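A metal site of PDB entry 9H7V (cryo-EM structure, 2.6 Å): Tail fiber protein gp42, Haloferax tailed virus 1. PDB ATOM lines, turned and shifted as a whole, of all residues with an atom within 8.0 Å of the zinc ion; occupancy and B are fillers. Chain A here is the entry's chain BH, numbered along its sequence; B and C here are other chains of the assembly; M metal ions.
Within 4 Å of the zinc ion: His 246 of chain A, His 250 of chain A, His 246 of chain B and His 250 of chain B.
The zinc ion is bound by a ring nitrogen (NE2) of His 250 of chain A, a ring nitrogen (NE2) of His 246 of chain A, a ring nitrogen (NE2) of His 246 of chain B and a ring nitrogen (NE2) of His 250 of chain B.
The zinc ion has four donor atoms within binding distance.
O of His 246 of chain A is in hydrogen-bond range of OG of Ser 249 of chain A (2.7 Å).
A ring nitrogen (ND1) of His 246 of chain B is in hydrogen-bond range of the backbone carbonyl oxygen of Lys 244 of chain B.
A ring nitrogen (ND1) of His 250 of chain A sits at hydrogen-bond distance from the backbone carbonyl oxygen (O) of Asp 256 of chain A (2.9 Å).
The backbone NH (N) of His 246 of chain B lies within hydrogen-bond range of the side-chain carboxylate (OD2) of Asp 256 of chain A, 2.7 Å away.
The backbone NH of His 246 of chain A lies within hydrogen-bond range of the side-chain carboxylate of Asp 256 of chain C, 2.9 Å away.
O of His 246 of chain B is in hydrogen-bond range of OG of Ser 249 of chain B, 2.7 Å away.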
ATOM      1  N   PRO A 243      -3.262  15.254  22.389  1.00  0.00           N
ATOM      2  CA  PRO A 243      -3.339  16.579  21.771  1.00  0.00           C
ATOM      3  C   PRO A 243      -2.408  17.635  22.365  1.00  0.00           C
ATOM      4  O   PRO A 243      -2.188  17.663  23.573  1.00  0.00           O
ATOM      5  CB  PRO A 243      -4.819  16.983  21.985  1.00  0.00           C
ATOM      6  CG  PRO A 243      -5.220  16.249  23.249  1.00  0.00           C
ATOM      7  CD  PRO A 243      -4.408  14.972  23.270  1.00  0.00           C
ATOM      8  N   LYS A 244      -1.859  18.470  21.474  1.00  0.00           N
ATOM      9  CA  LYS A 244      -1.191  19.716  21.785  1.00  0.00           C
ATOM     10  C   LYS A 244      -2.216  20.658  22.435  1.00  0.00           C
ATOM     11  O   LYS A 244      -3.401  20.587  22.116  1.00  0.00           O
ATOM     12  CB  LYS A 244      -0.622  20.277  20.480  1.00  0.00           C
ATOM     13  CG  LYS A 244       0.325  21.462  20.553  1.00  0.00           C
ATOM     14  CD  LYS A 244       1.048  21.652  19.241  1.00  0.00           C
ATOM     15  CE  LYS A 244       1.310  23.098  18.879  1.00  0.00           C
ATOM     16  NZ  LYS A 244       1.606  23.248  17.432  1.00  0.00           N
ATOM     17  N   HIS A 246      -4.758  23.444  23.615  1.00  0.00           N
ATOM     18  CA  HIS A 246      -5.787  23.786  22.637  1.00  0.00           C
ATOM     19  C   HIS A 246      -6.939  24.632  23.187  1.00  0.00           C
ATOM     20  O   HIS A 246      -7.580  25.343  22.412  1.00  0.00           O
ATOM     21  CB  HIS A 246      -6.290  22.510  21.959  1.00  0.00           C
ATOM     22  CG  HIS A 246      -7.421  21.840  22.670  1.00  0.00           C
ATOM     23  ND1 HIS A 246      -7.239  20.771  23.521  1.00  0.00           N
ATOM     24  CD2 HIS A 246      -8.737  22.113  22.673  1.00  0.00           C
ATOM     25  CE1 HIS A 246      -8.416  20.405  23.999  1.00  0.00           C
ATOM     26  NE2 HIS A 246      -9.354  21.221  23.489  1.00  0.00           N
ATOM     27  N   ALA A 247      -7.209  24.559  24.501  1.00  0.00           N
ATOM     28  CA  ALA A 247      -8.491  24.931  25.096  1.00  0.00           C
ATOM     29  C   ALA A 247      -8.937  26.355  24.767  1.00  0.00           C
ATOM     30  O   ALA A 247     -10.145  26.623  24.737  1.00  0.00           O
ATOM     31  CB  ALA A 247      -8.472  24.677  26.582  1.00  0.00           C
ATOM     32  N   ALA A 248      -7.967  27.259  24.526  1.00  0.00           N
ATOM     33  CA  ALA A 248      -8.216  28.649  24.165  1.00  0.00           C
ATOM     34  C   ALA A 248      -9.095  28.775  22.923  1.00  0.00           C
ATOM     35  O   ALA A 248      -9.781  29.788  22.756  1.00  0.00           O
ATOM     36  CB  ALA A 248      -6.891  29.361  23.976  1.00  0.00           C
ATOM     37  N   SER A 249      -9.082  27.747  22.066  1.00  0.00           N
ATOM     38  CA  SER A 249      -9.835  27.718  20.821  1.00  0.00           C
ATOM     39  C   SER A 249     -11.331  27.501  21.062  1.00  0.00           C
ATOM     40  O   SER A 249     -12.121  27.548  20.114  1.00  0.00           O
ATOM     41  CB  SER A 249      -9.272  26.694  19.861  1.00  0.00           C
ATOM     42  OG  SER A 249      -9.412  25.376  20.392  1.00  0.00           O
ATOM     43  N   HIS A 250     -11.714  27.284  22.325  1.00  0.00           N
ATOM     44  CA  HIS A 250     -13.112  27.083  22.694  1.00  0.00           C
ATOM     45  C   HIS A 250     -13.737  28.356  23.266  1.00  0.00           C
ATOM     46  O   HIS A 250     -14.829  28.293  23.841  1.00  0.00           O
ATOM     47  CB  HIS A 250     -13.283  25.869  23.624  1.00  0.00           C
ATOM     48  CG  HIS A 250     -12.780  24.581  23.058  1.00  0.00           C
ATOM     49  ND1 HIS A 250     -13.113  24.142  21.793  1.00  0.00           N
ATOM     50  CD2 HIS A 250     -11.987  23.628  23.598  1.00  0.00           C
ATOM     51  CE1 HIS A 250     -12.531  22.976  21.572  1.00  0.00           C
ATOM     52  NE2 HIS A 250     -11.840  22.643  22.678  1.00  0.00           N
ATOM     53  N   ASP A 256     -14.042  26.536  17.267  1.00  0.00           N
ATOM     54  CA  ASP A 256     -14.690  25.295  17.691  1.00  0.00           C
ATOM     55  C   ASP A 256     -15.435  25.519  19.012  1.00  0.00           C
ATOM     56  O   ASP A 256     -14.800  25.713  20.044  1.00  0.00           O
ATOM     57  CB  ASP A 256     -13.652  24.157  17.754  1.00  0.00           C
ATOM     58  CG  ASP A 256     -14.203  22.745  17.703  1.00  0.00           C
ATOM     59  OD1 ASP A 256     -15.375  22.575  17.312  1.00  0.00           O
ATOM     60  OD2 ASP A 256     -13.451  21.814  18.052  1.00  0.00           O
ATOM     61  N   ILE A 258     -18.143  25.374  22.298  1.00  0.00           N
ATOM     62  CA  ILE A 258     -18.845  24.707  23.396  1.00  0.00           C
ATOM     63  C   ILE A 258     -19.529  25.779  24.259  1.00  0.00           C
ATOM     64  O   ILE A 258     -19.025  26.897  24.364  1.00  0.00           O
ATOM     65  CB  ILE A 258     -17.901  23.775  24.197  1.00  0.00           C
ATOM     66  CG1 ILE A 258     -18.662  22.850  25.168  1.00  0.00           C
ATOM     67  CG2 ILE A 258     -16.790  24.545  24.901  1.00  0.00           C
ATOM     68  CD1 ILE A 258     -19.353  21.680  24.513  1.00  0.00           C
ATOM     69  N   PRO B 243      -4.859  19.275  17.570  1.00  0.00           N
ATOM     70  CA  PRO B 243      -6.141  18.563  17.532  1.00  0.00           C
ATOM     71  C   PRO B 243      -7.117  19.114  16.489  1.00  0.00           C
ATOM     72  O   PRO B 243      -7.248  20.328  16.319  1.00  0.00           O
ATOM     73  CB  PRO B 243      -6.678  18.693  18.958  1.00  0.00           C
ATOM     74  CG  PRO B 243      -6.050  19.964  19.492  1.00  0.00           C
ATOM     75  CD  PRO B 243      -4.725  20.110  18.780  1.00  0.00           C
ATOM     76  N   LYS B 244      -7.791  18.176  15.817  1.00  0.00           N
ATOM     77  CA  LYS B 244      -8.856  18.377  14.836  1.00  0.00           C
ATOM     78  C   LYS B 244     -10.093  18.935  15.544  1.00  0.00           C
ATOM     79  O   LYS B 244     -10.121  18.973  16.776  1.00  0.00           O
ATOM     80  CB  LYS B 244      -9.167  16.990  14.254  1.00  0.00           C
ATOM     81  CG  LYS B 244      -9.830  16.903  12.885  1.00  0.00           C
ATOM     82  CD  LYS B 244      -9.628  15.515  12.282  1.00  0.00           C
ATOM     83  CE  LYS B 244     -10.872  14.923  11.649  1.00  0.00           C
ATOM     84  NZ  LYS B 244     -10.691  13.489  11.316  1.00  0.00           N
ATOM     85  N   ALA B 245     -11.113  19.361  14.776  1.00  0.00           N
ATOM     86  CA  ALA B 245     -12.366  19.856  15.324  1.00  0.00           C
ATOM     87  C   ALA B 245     -13.045  18.785  16.172  1.00  0.00           C
ATOM     88  O   ALA B 245     -13.227  17.653  15.707  1.00  0.00           O
ATOM     89  CB  ALA B 245     -13.262  20.338  14.205  1.00  0.00           C
ATOM     90  N   HIS B 246     -13.418  19.140  17.415  1.00  0.00           N
ATOM     91  CA  HIS B 246     -13.704  18.138  18.435  1.00  0.00           C
ATOM     92  C   HIS B 246     -14.570  18.643  19.601  1.00  0.00           C
ATOM     93  O   HIS B 246     -14.910  17.836  20.468  1.00  0.00           O
ATOM     94  CB  HIS B 246     -12.377  17.598  18.997  1.00  0.00           C
ATOM     95  CG  HIS B 246     -11.711  18.588  19.877  1.00  0.00           C
ATOM     96  ND1 HIS B 246     -10.935  19.611  19.394  1.00  0.00           N
ATOM     97  CD2 HIS B 246     -11.758  18.752  21.218  1.00  0.00           C
ATOM     98  CE1 HIS B 246     -10.505  20.358  20.394  1.00  0.00           C
ATOM     99  NE2 HIS B 246     -11.000  19.844  21.530  1.00  0.00           N
ATOM    100  N   ALA B 247     -14.913  19.945  19.647  1.00  0.00           N
ATOM    101  CA  ALA B 247     -15.430  20.604  20.849  1.00  0.00           C
ATOM    102  C   ALA B 247     -16.621  19.883  21.497  1.00  0.00           C
ATOM    103  O   ALA B 247     -16.799  19.976  22.711  1.00  0.00           O
ATOM    104  CB  ALA B 247     -15.747  22.047  20.572  1.00  0.00           C
ATOM    105  N   ALA B 248     -17.428  19.191  20.675  1.00  0.00           N
ATOM    106  CA  ALA B 248     -18.601  18.455  21.127  1.00  0.00           C
ATOM    107  C   ALA B 248     -18.242  17.354  22.119  1.00  0.00           C
ATOM    108  O   ALA B 248     -19.114  16.846  22.822  1.00  0.00           O
ATOM    109  CB  ALA B 248     -19.339  17.898  19.919  1.00  0.00           C
ATOM    110  N   SER B 249     -16.951  16.994  22.182  1.00  0.00           N
ATOM    111  CA  SER B 249     -16.447  15.979  23.111  1.00  0.00           C
ATOM    112  C   SER B 249     -16.267  16.561  24.522  1.00  0.00           C
ATOM    113  O   SER B 249     -15.829  15.857  25.427  1.00  0.00           O
ATOM    114  CB  SER B 249     -15.182  15.331  22.597  1.00  0.00           C
ATOM    115  OG  SER B 249     -14.121  16.267  22.499  1.00  0.00           O
ATOM    116  N   HIS B 250     -16.637  17.846  24.693  1.00  0.00           N
ATOM    117  CA  HIS B 250     -16.638  18.501  25.991  1.00  0.00           C
ATOM    118  C   HIS B 250     -18.057  18.573  26.559  1.00  0.00           C
ATOM    119  O   HIS B 250     -18.326  19.395  27.442  1.00  0.00           O
ATOM    120  CB  HIS B 250     -15.923  19.873  25.917  1.00  0.00           C
ATOM    121  CG  HIS B 250     -14.536  19.846  25.377  1.00  0.00           C
ATOM    122  ND1 HIS B 250     -13.523  19.096  25.942  1.00  0.00           N
ATOM    123  CD2 HIS B 250     -13.964  20.513  24.348  1.00  0.00           C
ATOM    124  CE1 HIS B 250     -12.409  19.271  25.275  1.00  0.00           C
ATOM    125  NE2 HIS B 250     -12.644  20.132  24.291  1.00  0.00           N
ATOM    126  N   PRO C 243      -8.026  13.837  18.575  1.00  0.00           N
ATOM    127  CA  PRO C 243      -7.444  13.830  19.922  1.00  0.00           C
ATOM    128  C   PRO C 243      -7.745  12.551  20.714  1.00  0.00           C
ATOM    129  O   PRO C 243      -8.850  12.024  20.657  1.00  0.00           O
ATOM    130  CB  PRO C 243      -8.069  15.063  20.593  1.00  0.00           C
ATOM    131  CG  PRO C 243      -9.409  15.232  19.898  1.00  0.00           C
ATOM    132  CD  PRO C 243      -9.195  14.740  18.486  1.00  0.00           C
ATOM    133  N   HIS C 246      -8.675  13.038  26.977  1.00  0.00           N
ATOM    134  CA  HIS C 246      -7.921  14.244  27.331  1.00  0.00           C
ATOM    135  C   HIS C 246      -8.577  15.162  28.381  1.00  0.00           C
ATOM    136  O   HIS C 246      -7.849  15.813  29.119  1.00  0.00           O
ATOM    137  CB  HIS C 246      -7.569  15.041  26.063  1.00  0.00           C
ATOM    138  CG  HIS C 246      -8.761  15.613  25.369  1.00  0.00           C
ATOM    139  ND1 HIS C 246      -9.496  14.898  24.447  1.00  0.00           N
ATOM    140  CD2 HIS C 246      -9.358  16.811  25.485  1.00  0.00           C
ATOM    141  CE1 HIS C 246     -10.486  15.639  24.006  1.00  0.00           C
ATOM    142  NE2 HIS C 246     -10.432  16.824  24.631  1.00  0.00           N
ATOM    143  N   ALA C 247      -9.909  15.223  28.426  1.00  0.00           N
ATOM    144  CA  ALA C 247     -10.672  16.373  28.908  1.00  0.00           C
ATOM    145  C   ALA C 247     -10.359  16.815  30.348  1.00  0.00           C
ATOM    146  O   ALA C 247     -10.740  17.919  30.745  1.00  0.00           O
ATOM    147  CB  ALA C 247     -12.153  16.153  28.689  1.00  0.00           C
ATOM    148  N   SER C 249      -7.584  17.643  31.269  1.00  0.00           N
ATOM    149  CA  SER C 249      -6.548  18.643  31.050  1.00  0.00           C
ATOM    150  C   SER C 249      -7.045  20.055  31.393  1.00  0.00           C
ATOM    151  O   SER C 249      -6.239  20.926  31.709  1.00  0.00           O
ATOM    152  CB  SER C 249      -6.035  18.567  29.634  1.00  0.00           C
ATOM    153  OG  SER C 249      -7.069  18.866  28.697  1.00  0.00           O
ATOM    154  N   HIS C 250      -8.366  20.263  31.347  1.00  0.00           N
ATOM    155  CA  HIS C 250      -8.983  21.567  31.546  1.00  0.00           C
ATOM    156  C   HIS C 250      -9.218  21.879  33.026  1.00  0.00           C
ATOM    157  O   HIS C 250      -9.750  22.950  33.337  1.00  0.00           O
ATOM    158  CB  HIS C 250     -10.264  21.716  30.704  1.00  0.00           C
ATOM    159  CG  HIS C 250     -10.133  21.242  29.293  1.00  0.00           C
ATOM    160  ND1 HIS C 250      -9.217  21.781  28.411  1.00  0.00           N
ATOM    161  CD2 HIS C 250     -10.815  20.299  28.610  1.00  0.00           C
ATOM    162  CE1 HIS C 250      -9.321  21.178  27.250  1.00  0.00           C
ATOM    163  NE2 HIS C 250     -10.288  20.259  27.341  1.00  0.00           N
ATOM    164  N   ASP C 256      -3.824  23.169  30.033  1.00  0.00           N
ATOM    165  CA  ASP C 256      -4.750  23.230  28.906  1.00  0.00           C
ATOM    166  C   ASP C 256      -6.000  23.989  29.333  1.00  0.00           C
ATOM    167  O   ASP C 256      -7.111  23.467  29.223  1.00  0.00           O
ATOM    168  CB  ASP C 256      -5.001  21.813  28.370  1.00  0.00           C
ATOM    169  CG  ASP C 256      -5.673  21.709  27.015  1.00  0.00           C
ATOM    170  OD1 ASP C 256      -5.645  22.697  26.244  1.00  0.00           O
ATOM    171  OD2 ASP C 256      -6.212  20.615  26.713  1.00  0.00           O
ATOM    172  N   ILE C 258      -9.081  26.632  29.983  1.00  0.00           N
ATOM    173  CA  ILE C 258     -10.109  27.547  29.516  1.00  0.00           C
ATOM    174  C   ILE C 258     -10.966  27.944  30.715  1.00  0.00           C
ATOM    175  O   ILE C 258     -11.337  27.091  31.524  1.00  0.00           O
ATOM    176  CB  ILE C 258     -10.930  26.949  28.336  1.00  0.00           C
ATOM    177  CG1 ILE C 258     -11.907  27.966  27.725  1.00  0.00           C
ATOM    178  CG2 ILE C 258     -11.619  25.641  28.699  1.00  0.00           C
ATOM    179  CD1 ILE C 258     -11.260  28.980  26.798  1.00  0.00           C
HETATM  180 ZN    ZN M   1     -11.225  20.956  23.095  1.00  0.00          ZN
